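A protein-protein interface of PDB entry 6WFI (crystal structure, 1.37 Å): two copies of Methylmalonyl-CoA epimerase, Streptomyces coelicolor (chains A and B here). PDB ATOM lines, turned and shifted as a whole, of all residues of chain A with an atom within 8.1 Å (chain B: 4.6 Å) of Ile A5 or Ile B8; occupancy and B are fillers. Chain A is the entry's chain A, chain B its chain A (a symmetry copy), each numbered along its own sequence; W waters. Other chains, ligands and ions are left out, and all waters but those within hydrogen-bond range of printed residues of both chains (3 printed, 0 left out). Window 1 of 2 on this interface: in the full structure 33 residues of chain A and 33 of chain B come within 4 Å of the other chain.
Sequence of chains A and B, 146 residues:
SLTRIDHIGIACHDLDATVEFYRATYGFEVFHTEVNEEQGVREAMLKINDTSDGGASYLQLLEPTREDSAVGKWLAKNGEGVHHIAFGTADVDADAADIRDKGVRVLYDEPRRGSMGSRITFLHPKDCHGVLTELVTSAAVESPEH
OD1 of Asn B49 sits at hydrogen-bond distance from N of Ile A5 (3.0 Å).
O of Thr A3 sits close to O of Ile B48.
The backbone carbonyl oxygen of Ile A85 sits at hydrogen-bond distance from the backbone NH of Glu A134, at 2.8 Å.
The backbone NH (N) of Phe A87 is in hydrogen-bond range of the backbone carbonyl oxygen (O) of Glu A134.
O of Phe A87 sits at hydrogen-bond distance from N of Val A136, at 2.9 Å.
The backbone carbonyl oxygen of Tyr B58 lies within hydrogen-bond range of the backbone NH of Ile B8.
O of Ser B57 lies within hydrogen-bond range of N of Ile B48 (2.9 Å).
O of Asn B49 sits at hydrogen-bond distance from N of Ser B57, 2.9 Å away.
Of the printed residues of chain B, Ile A5 touches Ile B8 (3.95 Å), Ile B48 (3.7 Å), Asn B49 (3.0 Å), Ser B57 (3.99 Å) and Tyr B58 (3.8 Å).
Of the printed residues of chain A, Ser B57 touches Ile A5 (3.99 Å).
Of the printed residues of chain A, Asn B49 touches Thr A3, Arg A4, Ile A5 and Thr A51.
Of the printed residues of chain A, Tyr B58 touches Ile A5.
Of the printed residues of chain B, Thr A51 touches Asn B49 (3.4 Å).
Gly A88 touches none of the printed residues of chain B.
Asp A6 touches none of the printed residues of chain B.
The nearest printed residue of chain B that does not touch Ile A5 is Leu B59 (4.1 Å).
Water W1 lies within hydrogen-bond range of the side-chain hydroxyl (OG) of Ser A57 (2.6 Å), the side-chain hydroxyl (OG) of Ser B57 (2.6 Å), the side-chain amide nitrogen (ND2) of Asn A49 (3.0 Å) and the side-chain amide nitrogen (ND2) of Asn B49 (3.0 Å).
Water W3 bridges the backbone carbonyl oxygen (O) of Ile B48 (2.7 Å) and the backbone carbonyl oxygen (O) of Leu A2 (2.9 Å).
Water W2 lies within hydrogen-bond range of O of Thr A3 and O of Ile B48.
C of Arg A4 touches CG2 of Ile B48, 3.6 Å away.
Asn B49 touches Arg A4 (OD1 to CA, 3.2 Å).
Ile A5 touches Ile B8.
N of Ile A5 touches CG2 of Ile B48, at 3.7 Å.
Tyr B58 touches Ile A5 (O to CD1, 3.8 Å).
CG2 of Thr A51 touches ND2 of Asn B49, at 3.4 Å.
Val A82 touches Val B82.
Ile A85 touches Ile B8 (CG2 to CD1, 3.9 Å).
Val B82 touches Ile A85.
Leu B59 touches Phe A87 (CD1 to CZ, 3.8 Å).
Val B82 touches its own counterpart, Val A82.
Of the 14 pairs that touch across the chains among the printed residues, 1 has its exchanged pair printed and touching as well.
Of the 12 printed residues of chain B, 7 touch a printed residue of chain A.
Hydrophobic or aromatic side chains of chain B that line the printed part of chain A: Ile B8, Ile B48, Leu B59 and Val B82.
Along chain B the printed residues that touch a printed residue of chain A span positions 8 to 82.
Along chain A the printed residues that touch a printed residue of chain B span positions 3 to 87.
Among the printed residues, 14 pairs touch across the chains.
Among the printed residues, no Asp or Glu carboxylate lies within 4 Å of a Lys or Arg side-chain nitrogen of the other chain.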
ATOM      1  N   LEU A   2     -17.121 -24.012  19.055  1.00  0.00           N
ATOM      2  CA  LEU A   2     -18.530 -24.356  19.430  1.00  0.00           C
ATOM      3  C   LEU A   2     -18.476 -25.308  20.619  1.00  0.00           C
ATOM      4  O   LEU A   2     -17.986 -26.441  20.506  1.00  0.00           O
ATOM      5  CB  LEU A   2     -19.251 -25.011  18.264  1.00  0.00           C
ATOM      6  CG  LEU A   2     -19.304 -24.196  16.982  1.00  0.00           C
ATOM      7  CD1 LEU A   2     -20.088 -24.975  15.951  1.00  0.00           C
ATOM      8  CD2 LEU A   2     -19.838 -22.767  17.203  1.00  0.00           C
ATOM      9  N   THR A   3     -18.933 -24.854  21.774  1.00  0.00           N
ATOM     10  CA  THR A   3     -18.727 -25.514  23.050  1.00  0.00           C
ATOM     11  C   THR A   3     -19.970 -26.147  23.642  1.00  0.00           C
ATOM     12  O   THR A   3     -19.884 -26.795  24.703  1.00  0.00           O
ATOM     13  CB  THR A   3     -18.048 -24.570  24.025  1.00  0.00           C
ATOM     14  OG1 THR A   3     -18.819 -23.384  24.145  1.00  0.00           O
ATOM     15  CG2 THR A   3     -16.629 -24.302  23.562  1.00  0.00           C
ATOM     16  N   ARG A   4     -21.157 -25.942  23.064  1.00  0.00           N
ATOM     17  CA  ARG A   4     -22.399 -26.595  23.554  1.00  0.00           C
ATOM     18  C   ARG A   4     -23.414 -26.650  22.424  1.00  0.00           C
ATOM     19  O   ARG A   4     -23.357 -25.892  21.460  1.00  0.00           O
ATOM     20  CB  ARG A   4     -22.983 -25.803  24.736  1.00  0.00           C
ATOM     21  CG  ARG A   4     -23.519 -24.454  24.393  1.00  0.00           C
ATOM     22  CD  ARG A   4     -24.128 -23.717  25.577  1.00  0.00           C
ATOM     23  NE  ARG A   4     -24.614 -22.399  25.198  1.00  0.00           N
ATOM     24  CZ  ARG A   4     -23.804 -21.358  24.983  1.00  0.00           C
ATOM     25  NH1 ARG A   4     -22.522 -21.436  25.276  1.00  0.00           N
ATOM     26  NH2 ARG A   4     -24.299 -20.232  24.533  1.00  0.00           N
ATOM     27  N   ILE A   5     -24.386 -27.508  22.669  1.00  0.00           N
ATOM     28  CA  ILE A   5     -25.704 -27.387  22.029  1.00  0.00           C
ATOM     29  C   ILE A   5     -26.407 -26.283  22.749  1.00  0.00           C
ATOM     30  O   ILE A   5     -26.701 -26.482  23.963  1.00  0.00           O
ATOM     31  CB  ILE A   5     -26.450 -28.699  21.983  1.00  0.00           C
ATOM     32  CG1 ILE A   5     -25.701 -29.725  21.140  1.00  0.00           C
ATOM     33  CG2 ILE A   5     -27.875 -28.466  21.495  1.00  0.00           C
ATOM     34  CD1 ILE A   5     -26.239 -31.138  21.181  1.00  0.00           C
ATOM     35  N   ASP A   6     -26.718 -25.157  22.205  1.00  0.00           N
ATOM     36  CA  ASP A   6     -27.434 -24.058  22.867  1.00  0.00           C
ATOM     37  C   ASP A   6     -28.915 -24.335  22.829  1.00  0.00           C
ATOM     38  O   ASP A   6     -29.593 -24.185  23.851  1.00  0.00           O
ATOM     39  CB  ASP A   6     -27.105 -22.699  22.263  1.00  0.00           C
ATOM     40  CG  ASP A   6     -27.680 -21.568  23.048  1.00  0.00           C
ATOM     41  OD1 ASP A   6     -27.034 -21.161  24.028  1.00  0.00           O
ATOM     42  OD2 ASP A   6     -28.777 -21.126  22.720  1.00  0.00           O
ATOM     43  N   HIS A   7     -29.491 -24.688  21.704  1.00  0.00           N
ATOM     44  CA  HIS A   7     -30.942 -24.974  21.695  1.00  0.00           C
ATOM     45  C   HIS A   7     -31.277 -25.776  20.465  1.00  0.00           C
ATOM     46  O   HIS A   7     -30.555 -25.858  19.456  1.00  0.00           O
ATOM     47  CB  HIS A   7     -31.767 -23.701  21.767  1.00  0.00           C
ATOM     48  CG  HIS A   7     -31.589 -22.691  20.674  1.00  0.00           C
ATOM     49  ND1 HIS A   7     -30.649 -21.676  20.749  1.00  0.00           N
ATOM     50  CD2 HIS A   7     -32.313 -22.455  19.551  1.00  0.00           C
ATOM     51  CE1 HIS A   7     -30.838 -20.867  19.669  1.00  0.00           C
ATOM     52  NE2 HIS A   7     -31.825 -21.315  18.938  1.00  0.00           N
ATOM     53  N   ILE A   8     -32.526 -26.282  20.499  1.00  0.00           N
ATOM     54  CA  ILE A   8     -33.207 -26.929  19.370  1.00  0.00           C
ATOM     55  C   ILE A   8     -34.358 -26.022  18.982  1.00  0.00           C
ATOM     56  O   ILE A   8     -35.196 -25.726  19.878  1.00  0.00           O
ATOM     57  CB  ILE A   8     -33.697 -28.337  19.748  1.00  0.00           C
ATOM     58  CG1 ILE A   8     -32.537 -29.187  20.270  1.00  0.00           C
ATOM     59  CG2 ILE A   8     -34.376 -28.967  18.506  1.00  0.00           C
ATOM     60  CD1 ILE A   8     -32.970 -30.513  20.880  1.00  0.00           C
ATOM     61  N   GLY A   9     -34.396 -25.519  17.773  1.00  0.00           N
ATOM     62  CA  GLY A   9     -35.490 -24.683  17.319  1.00  0.00           C
ATOM     63  C   GLY A   9     -36.600 -25.511  16.769  1.00  0.00           C
ATOM     64  O   GLY A   9     -36.365 -26.299  15.798  1.00  0.00           O
ATOM     65  N   ASN A  49     -31.293 -27.856  30.729  1.00  0.00           N
ATOM     66  CA  ASN A  49     -30.112 -28.158  31.557  1.00  0.00           C
ATOM     67  C   ASN A  49     -29.132 -27.027  31.426  1.00  0.00           C
ATOM     68  O   ASN A  49     -29.154 -26.249  30.475  1.00  0.00           O
ATOM     69  CB  ASN A  49     -29.495 -29.512  31.232  1.00  0.00           C
ATOM     70  CG  ASN A  49     -29.110 -29.691  29.780  1.00  0.00           C
ATOM     71  OD1 ASN A  49     -29.935 -30.116  28.967  1.00  0.00           O
ATOM     72  ND2 ASN A  49     -27.873 -29.318  29.448  1.00  0.00           N
ATOM     73  N   ASP A  50     -28.173 -26.976  32.360  1.00  0.00           N
ATOM     74  CA  ASP A  50     -26.960 -26.180  32.208  1.00  0.00           C
ATOM     75  C   ASP A  50     -25.895 -27.039  31.543  1.00  0.00           C
ATOM     76  O   ASP A  50     -25.987 -28.249  31.519  1.00  0.00           O
ATOM     77  CB  ASP A  50     -26.529 -25.634  33.609  1.00  0.00           C
ATOM     78  CG  ASP A  50     -27.434 -24.557  34.116  1.00  0.00           C
ATOM     79  OD1 ASP A  50     -27.552 -23.534  33.558  1.00  0.00           O
ATOM     80  OD2 ASP A  50     -28.038 -24.834  35.211  1.00  0.00           O
ATOM     81  N   THR A  51     -24.868 -26.337  31.030  1.00  0.00           N
ATOM     82  CA  THR A  51     -23.800 -27.017  30.242  1.00  0.00           C
ATOM     83  C   THR A  51     -22.398 -26.688  30.798  1.00  0.00           C
ATOM     84  O   THR A  51     -22.206 -25.666  31.462  1.00  0.00           O
ATOM     85  CB  THR A  51     -23.922 -26.663  28.751  1.00  0.00           C
ATOM     86  OG1 THR A  51     -23.834 -25.265  28.586  1.00  0.00           O
ATOM     87  CG2 THR A  51     -25.254 -27.124  28.182  1.00  0.00           C
ATOM     88  N   ASP A  53     -19.715 -25.589  29.542  1.00  0.00           N
ATOM     89  CA  ASP A  53     -19.039 -24.331  29.128  1.00  0.00           C
ATOM     90  C   ASP A  53     -19.565 -23.126  29.866  1.00  0.00           C
ATOM     91  O   ASP A  53     -19.226 -21.995  29.529  1.00  0.00           O
ATOM     92  CB  ASP A  53     -19.184 -24.189  27.615  1.00  0.00           C
ATOM     93  CG  ASP A  53     -20.609 -23.951  27.117  1.00  0.00           C
ATOM     94  OD1 ASP A  53     -21.512 -24.107  27.948  1.00  0.00           O
ATOM     95  OD2 ASP A  53     -20.727 -23.567  25.957  1.00  0.00           O
ATOM     96  N   GLY A  55     -22.798 -22.336  29.880  1.00  0.00           N
ATOM     97  CA  GLY A  55     -24.068 -21.967  29.272  1.00  0.00           C
ATOM     98  C   GLY A  55     -25.181 -22.898  29.670  1.00  0.00           C
ATOM     99  O   GLY A  55     -25.243 -23.438  30.764  1.00  0.00           O
ATOM    100  N   ALA A  56     -26.179 -22.974  28.774  1.00  0.00           N
ATOM    101  CA  ALA A  56     -27.381 -23.761  29.021  1.00  0.00           C
ATOM    102  C   ALA A  56     -27.881 -24.302  27.697  1.00  0.00           C
ATOM    103  O   ALA A  56     -27.476 -23.817  26.626  1.00  0.00           O
ATOM    104  CB  ALA A  56     -28.428 -22.943  29.705  1.00  0.00           C
ATOM    105  N   SER A  57     -28.780 -25.226  27.775  1.00  0.00           N
ATOM    106  CA  SER A  57     -29.462 -25.822  26.596  1.00  0.00           C
ATOM    107  C   SER A  57     -30.938 -25.674  26.763  1.00  0.00           C
ATOM    108  O   SER A  57     -31.492 -26.005  27.839  1.00  0.00           O
ATOM    109  CB  SER A  57     -29.184 -27.267  26.365  1.00  0.00           C
ATOM    110  OG  SER A  57     -27.793 -27.512  26.147  1.00  0.00           O
ATOM    111  N   TYR A  58     -31.580 -25.238  25.721  1.00  0.00           N
ATOM    112  CA  TYR A  58     -32.991 -24.916  25.680  1.00  0.00           C
ATOM    113  C   TYR A  58     -33.693 -25.603  24.566  1.00  0.00           C
ATOM    114  O   TYR A  58     -33.108 -25.954  23.497  1.00  0.00           O
ATOM    115  CB  TYR A  58     -33.227 -23.419  25.451  1.00  0.00           C
ATOM    116  CG  TYR A  58     -32.524 -22.488  26.383  1.00  0.00           C
ATOM    117  CD1 TYR A  58     -31.205 -22.087  26.154  1.00  0.00           C
ATOM    118  CD2 TYR A  58     -33.103 -22.001  27.563  1.00  0.00           C
ATOM    119  CE1 TYR A  58     -30.555 -21.171  26.971  1.00  0.00           C
ATOM    120  CE2 TYR A  58     -32.440 -21.112  28.391  1.00  0.00           C
ATOM    121  CZ  TYR A  58     -31.189 -20.698  28.098  1.00  0.00           C
ATOM    122  OH  TYR A  58     -30.529 -19.802  28.929  1.00  0.00           O
ATOM    123  N   VAL A  82     -38.978 -30.063  14.098  1.00  0.00           N
ATOM    124  CA  VAL A  82     -37.664 -29.428  14.305  1.00  0.00           C
ATOM    125  C   VAL A  82     -37.288 -28.588  13.130  1.00  0.00           C
ATOM    126  O   VAL A  82     -37.284 -29.098  11.973  1.00  0.00           O
ATOM    127  CB  VAL A  82     -36.580 -30.451  14.588  1.00  0.00           C
ATOM    128  CG1 VAL A  82     -35.244 -29.745  14.754  1.00  0.00           C
ATOM    129  CG2 VAL A  82     -36.866 -31.273  15.814  1.00  0.00           C
ATOM    130  N   HIS A  84     -34.405 -26.052  13.330  1.00  0.00           N
ATOM    131  CA  HIS A  84     -32.956 -25.790  13.300  1.00  0.00           C
ATOM    132  C   HIS A  84     -32.307 -26.288  14.568  1.00  0.00           C
ATOM    133  O   HIS A  84     -33.016 -26.588  15.550  1.00  0.00           O
ATOM    134  CB  HIS A  84     -32.637 -24.310  13.048  1.00  0.00           C
ATOM    135  CG  HIS A  84     -33.058 -23.368  14.133  1.00  0.00           C
ATOM    136  ND1 HIS A  84     -34.309 -22.768  14.108  1.00  0.00           N
ATOM    137  CD2 HIS A  84     -32.379 -22.812  15.170  1.00  0.00           C
ATOM    138  CE1 HIS A  84     -34.322 -21.899  15.162  1.00  0.00           C
ATOM    139  NE2 HIS A  84     -33.185 -21.895  15.812  1.00  0.00           N
ATOM    140  N   ILE A  85     -31.013 -26.332  14.594  1.00  0.00           N
ATOM    141  CA  ILE A  85     -30.219 -26.604  15.820  1.00  0.00           C
ATOM    142  C   ILE A  85     -29.290 -25.458  16.001  1.00  0.00           C
ATOM    143  O   ILE A  85     -28.850 -24.829  15.012  1.00  0.00           O
ATOM    144  CB  ILE A  85     -29.529 -27.956  15.739  1.00  0.00           C
ATOM    145  CG1 ILE A  85     -28.402 -27.940  14.803  1.00  0.00           C
ATOM    146  CG2 ILE A  85     -30.523 -29.035  15.418  1.00  0.00           C
ATOM    147  CD1 ILE A  85     -27.631 -29.291  14.856  1.00  0.00           C
ATOM    148  N   ALA A  86     -28.914 -25.154  17.203  1.00  0.00           N
ATOM    149  CA  ALA A  86     -28.021 -24.045  17.537  1.00  0.00           C
ATOM    150  C   ALA A  86     -26.878 -24.463  18.418  1.00  0.00           C
ATOM    151  O   ALA A  86     -27.117 -25.130  19.431  1.00  0.00           O
ATOM    152  CB  ALA A  86     -28.791 -22.931  18.194  1.00  0.00           C
ATOM    153  N   PHE A  87     -25.693 -24.047  18.085  1.00  0.00           N
ATOM    154  CA  PHE A  87     -24.458 -24.286  18.842  1.00  0.00           C
ATOM    155  C   PHE A  87     -24.030 -22.983  19.505  1.00  0.00           C
ATOM    156  O   PHE A  87     -24.012 -21.946  18.856  1.00  0.00           O
ATOM    157  CB  PHE A  87     -23.334 -24.822  17.946  1.00  0.00           C
ATOM    158  CG  PHE A  87     -23.636 -26.144  17.345  1.00  0.00           C
ATOM    159  CD1 PHE A  87     -23.687 -27.289  18.077  1.00  0.00           C
ATOM    160  CD2 PHE A  87     -23.881 -26.250  15.994  1.00  0.00           C
ATOM    161  CE1 PHE A  87     -23.997 -28.528  17.530  1.00  0.00           C
ATOM    162  CE2 PHE A  87     -24.195 -27.496  15.418  1.00  0.00           C
ATOM    163  CZ  PHE A  87     -24.292 -28.610  16.209  1.00  0.00           C
ATOM    164  N   GLY A  88     -23.626 -23.077  20.758  1.00  0.00           N
ATOM    165  CA  GLY A  88     -23.092 -21.912  21.485  1.00  0.00           C
ATOM    166  C   GLY A  88     -21.605 -21.784  21.366  1.00  0.00           C
ATOM    167  O   GLY A  88     -20.875 -22.784  21.238  1.00  0.00           O
ATOM    168  N   THR A  89     -21.158 -20.536  21.452  1.00  0.00           N
ATOM    169  CA  THR A  89     -19.741 -20.142  21.324  1.00  0.00           C
ATOM    170  C   THR A  89     -19.582 -18.875  22.126  1.00  0.00           C
ATOM    171  O   THR A  89     -20.470 -18.060  22.169  1.00  0.00           O
ATOM    172  CB  THR A  89     -19.357 -20.053  19.846  1.00  0.00           C
ATOM    173  OG1 THR A  89     -18.096 -19.295  19.814  1.00  0.00           O
ATOM    174  CG2 THR A  89     -20.340 -19.339  19.009  1.00  0.00           C
ATOM    175  N   VAL A 131     -29.271 -29.596   7.580  1.00  0.00           N
ATOM    176  CA  VAL A 131     -29.599 -29.070   8.933  1.00  0.00           C
ATOM    177  C   VAL A 131     -29.327 -27.586   8.939  1.00  0.00           C
ATOM    178  O   VAL A 131     -28.185 -27.121   8.794  1.00  0.00           O
ATOM    179  CB  VAL A 131     -28.774 -29.806   9.978  1.00  0.00           C
ATOM    180  CG1 VAL A 131     -29.059 -29.199  11.375  1.00  0.00           C
ATOM    181  CG2 VAL A 131     -29.063 -31.298   9.966  1.00  0.00           C
ATOM    182  N   GLU A 134     -27.564 -22.800  13.518  1.00  0.00           N
ATOM    183  CA  GLU A 134     -27.339 -21.478  14.094  1.00  0.00           C
ATOM    184  C   GLU A 134     -26.113 -21.532  14.999  1.00  0.00           C
ATOM    185  O   GLU A 134     -25.829 -22.529  15.646  1.00  0.00           O
ATOM    186  CB  GLU A 134     -28.547 -21.067  14.910  1.00  0.00           C
ATOM    187  CG  GLU A 134     -28.393 -19.808  15.703  1.00  0.00           C
ATOM    188  CD  GLU A 134     -29.567 -19.592  16.627  1.00  0.00           C
ATOM    189  OE1 GLU A 134     -30.655 -20.158  16.372  1.00  0.00           O
ATOM    190  OE2 GLU A 134     -29.404 -18.843  17.641  1.00  0.00           O
ATOM    191  N   VAL A 136     -24.506 -19.149  18.129  1.00  0.00           N
ATOM    192  CA  VAL A 136     -24.990 -18.094  19.055  1.00  0.00           C
ATOM    193  C   VAL A 136     -23.964 -17.839  20.160  1.00  0.00           C
ATOM    194  O   VAL A 136     -23.380 -18.741  20.722  1.00  0.00           O
ATOM    195  CB  VAL A 136     -26.384 -18.481  19.586  1.00  0.00           C
ATOM    196  CG1 VAL A 136     -26.374 -19.850  20.277  1.00  0.00           C
ATOM    197  CG2 VAL A 136     -26.884 -17.435  20.572  1.00  0.00           C
ATOM    198  N   HIS B   7     -29.315 -36.025  23.116  1.00  0.00           N
ATOM    199  CA  HIS B   7     -28.713 -35.921  21.770  1.00  0.00           C
ATOM    200  C   HIS B   7     -29.752 -35.414  20.805  1.00  0.00           C
ATOM    201  O   HIS B   7     -30.978 -35.439  21.008  1.00  0.00           O
ATOM    202  CB  HIS B   7     -28.131 -37.246  21.309  1.00  0.00           C
ATOM    203  CG  HIS B   7     -29.061 -38.417  21.203  1.00  0.00           C
ATOM    204  ND1 HIS B   7     -29.290 -39.280  22.262  1.00  0.00           N
ATOM    205  CD2 HIS B   7     -29.708 -38.947  20.135  1.00  0.00           C
ATOM    206  CE1 HIS B   7     -30.068 -40.296  21.796  1.00  0.00           C
ATOM    207  NE2 HIS B   7     -30.333 -40.116  20.529  1.00  0.00           N
ATOM    208  N   ILE B   8     -29.228 -35.063  19.613  1.00  0.00           N
ATOM    209  CA  ILE B   8     -30.006 -34.729  18.413  1.00  0.00           C
ATOM    210  C   ILE B   8     -29.731 -35.824  17.401  1.00  0.00           C
ATOM    211  O   ILE B   8     -28.528 -36.041  17.088  1.00  0.00           O
ATOM    212  CB  ILE B   8     -29.620 -33.344  17.867  1.00  0.00           C
ATOM    213  CG1 ILE B   8     -29.773 -32.278  18.954  1.00  0.00           C
ATOM    214  CG2 ILE B   8     -30.497 -33.047  16.625  1.00  0.00           C
ATOM    215  CD1 ILE B   8     -29.197 -30.921  18.572  1.00  0.00           C
ATOM    216  N   GLY B   9     -30.728 -36.549  16.957  1.00  0.00           N
ATOM    217  CA  GLY B   9     -30.545 -37.580  15.955  1.00  0.00           C
ATOM    218  C   GLY B   9     -30.640 -37.011  14.582  1.00  0.00           C
ATOM    219  O   GLY B   9     -31.700 -36.400  14.234  1.00  0.00           O
ATOM    220  N   ILE B  10     -29.618 -37.131  13.800  1.00  0.00           N
ATOM    221  CA  ILE B  10     -29.456 -36.521  12.465  1.00  0.00           C
ATOM    222  C   ILE B  10     -29.270 -37.605  11.448  1.00  0.00           C
ATOM    223  O   ILE B  10     -28.309 -38.375  11.551  1.00  0.00           O
ATOM    224  CB  ILE B  10     -28.286 -35.542  12.472  1.00  0.00           C
ATOM    225  CG1 ILE B  10     -28.594 -34.368  13.414  1.00  0.00           C
ATOM    226  CG2 ILE B  10     -27.968 -35.052  11.075  1.00  0.00           C
ATOM    227  CD1 ILE B  10     -27.442 -33.468  13.707  1.00  0.00           C
ATOM    228  N   ILE B  48     -20.708 -32.991  22.351  1.00  0.00           N
ATOM    229  CA  ILE B  48     -20.591 -31.547  22.271  1.00  0.00           C
ATOM    230  C   ILE B  48     -20.291 -30.943  23.609  1.00  0.00           C
ATOM    231  O   ILE B  48     -19.536 -29.963  23.675  1.00  0.00           O
ATOM    232  CB  ILE B  48     -21.845 -30.953  21.597  1.00  0.00           C
ATOM    233  CG1 ILE B  48     -22.205 -31.754  20.338  1.00  0.00           C
ATOM    234  CG2 ILE B  48     -21.569 -29.492  21.305  1.00  0.00           C
ATOM    235  CD1 ILE B  48     -21.115 -31.854  19.314  1.00  0.00           C
ATOM    236  N   ASN B  49     -20.878 -31.434  24.688  1.00  0.00           N
ATOM    237  CA  ASN B  49     -20.703 -30.841  26.026  1.00  0.00           C
ATOM    238  C   ASN B  49     -21.119 -31.851  27.057  1.00  0.00           C
ATOM    239  O   ASN B  49     -21.862 -32.792  26.788  1.00  0.00           O
ATOM    240  CB  ASN B  49     -21.427 -29.509  26.180  1.00  0.00           C
ATOM    241  CG  ASN B  49     -22.909 -29.566  25.881  1.00  0.00           C
ATOM    242  OD1 ASN B  49     -23.315 -29.405  24.727  1.00  0.00           O
ATOM    243  ND2 ASN B  49     -23.708 -29.846  26.911  1.00  0.00           N
ATOM    244  N   SER B  57     -24.304 -34.259  26.185  1.00  0.00           N
ATOM    245  CA  SER B  57     -25.118 -33.984  24.972  1.00  0.00           C
ATOM    246  C   SER B  57     -24.298 -34.273  23.760  1.00  0.00           C
ATOM    247  O   SER B  57     -23.135 -33.811  23.655  1.00  0.00           O
ATOM    248  CB  SER B  57     -25.620 -32.587  24.848  1.00  0.00           C
ATOM    249  OG  SER B  57     -26.459 -32.225  25.945  1.00  0.00           O
ATOM    250  N   TYR B  58     -24.886 -34.973  22.837  1.00  0.00           N
ATOM    251  CA  TYR B  58     -24.258 -35.463  21.627  1.00  0.00           C
ATOM    252  C   TYR B  58     -25.016 -35.089  20.407  1.00  0.00           C
ATOM    253  O   TYR B  58     -26.268 -34.881  20.413  1.00  0.00           O
ATOM    254  CB  TYR B  58     -24.178 -36.993  21.607  1.00  0.00           C
ATOM    255  CG  TYR B  58     -23.551 -37.639  22.799  1.00  0.00           C
ATOM    256  CD1 TYR B  58     -24.292 -37.916  23.951  1.00  0.00           C
ATOM    257  CD2 TYR B  58     -22.188 -37.957  22.871  1.00  0.00           C
ATOM    258  CE1 TYR B  58     -23.746 -38.576  25.045  1.00  0.00           C
ATOM    259  CE2 TYR B  58     -21.641 -38.587  23.976  1.00  0.00           C
ATOM    260  CZ  TYR B  58     -22.406 -38.898  25.043  1.00  0.00           C
ATOM    261  OH  TYR B  58     -21.855 -39.533  26.148  1.00  0.00           O
ATOM    262  N   LEU B  59     -24.330 -35.082  19.264  1.00  0.00           N
ATOM    263  CA  LEU B  59     -24.974 -35.258  17.948  1.00  0.00           C
ATOM    264  C   LEU B  59     -24.897 -36.702  17.598  1.00  0.00           C
ATOM    265  O   LEU B  59     -23.797 -37.316  17.677  1.00  0.00           O
ATOM    266  CB  LEU B  59     -24.267 -34.448  16.858  1.00  0.00           C
ATOM    267  CG  LEU B  59     -24.194 -32.963  17.155  1.00  0.00           C
ATOM    268  CD1 LEU B  59     -23.392 -32.291  16.045  1.00  0.00           C
ATOM    269  CD2 LEU B  59     -25.562 -32.305  17.309  1.00  0.00           C
ATOM    270  N   GLN B  60     -26.013 -37.342  17.295  1.00  0.00           N
ATOM    271  CA  GLN B  60     -26.082 -38.749  16.880  1.00  0.00           C
ATOM    272  C   GLN B  60     -26.327 -38.799  15.384  1.00  0.00           C
ATOM    273  O   GLN B  60     -27.457 -38.566  14.934  1.00  0.00           O
ATOM    274  CB  GLN B  60     -27.163 -39.451  17.657  1.00  0.00           C
ATOM    275  CG  GLN B  60     -27.254 -40.918  17.338  1.00  0.00           C
ATOM    276  CD  GLN B  60     -28.371 -41.521  18.120  1.00  0.00           C
ATOM    277  OE1 GLN B  60     -29.554 -41.276  17.817  1.00  0.00           O
ATOM    278  NE2 GLN B  60     -28.023 -42.227  19.194  1.00  0.00           N
ATOM    279  N   VAL B  82     -32.499 -33.367  10.485  1.00  0.00           N
ATOM    280  CA  VAL B  82     -32.823 -33.790  11.859  1.00  0.00           C
ATOM    281  C   VAL B  82     -33.933 -34.787  11.862  1.00  0.00           C
ATOM    282  O   VAL B  82     -35.024 -34.511  11.284  1.00  0.00           O
ATOM    283  CB  VAL B  82     -33.175 -32.610  12.746  1.00  0.00           C
ATOM    284  CG1 VAL B  82     -33.536 -33.107  14.136  1.00  0.00           C
ATOM    285  CG2 VAL B  82     -32.057 -31.610  12.849  1.00  0.00           C
ATOM    286  N   HIS B  84     -34.732 -36.877  14.989  1.00  0.00           N
ATOM    287  CA  HIS B  84     -35.372 -36.965  16.313  1.00  0.00           C
ATOM    288  C   HIS B  84     -34.593 -36.160  17.325  1.00  0.00           C
ATOM    289  O   HIS B  84     -33.442 -35.766  17.050  1.00  0.00           O
ATOM    290  CB  HIS B  84     -35.561 -38.417  16.773  1.00  0.00           C
ATOM    291  CG  HIS B  84     -34.298 -39.178  17.032  1.00  0.00           C
ATOM    292  ND1 HIS B  84     -33.693 -39.917  16.025  1.00  0.00           N
ATOM    293  CD2 HIS B  84     -33.612 -39.441  18.175  1.00  0.00           C
ATOM    294  CE1 HIS B  84     -32.648 -40.564  16.621  1.00  0.00           C
ATOM    295  NE2 HIS B  84     -32.574 -40.309  17.903  1.00  0.00           N
HETATM  296  O   HOH W   1     -26.674 -29.771  26.768  1.00  0.00           O
HETATM  297  O   HOH W   2     -17.658 -28.242  25.537  1.00  0.00           O
HETATM  298  O   HOH W   3     -17.809 -28.985  21.812  1.00  0.00           O
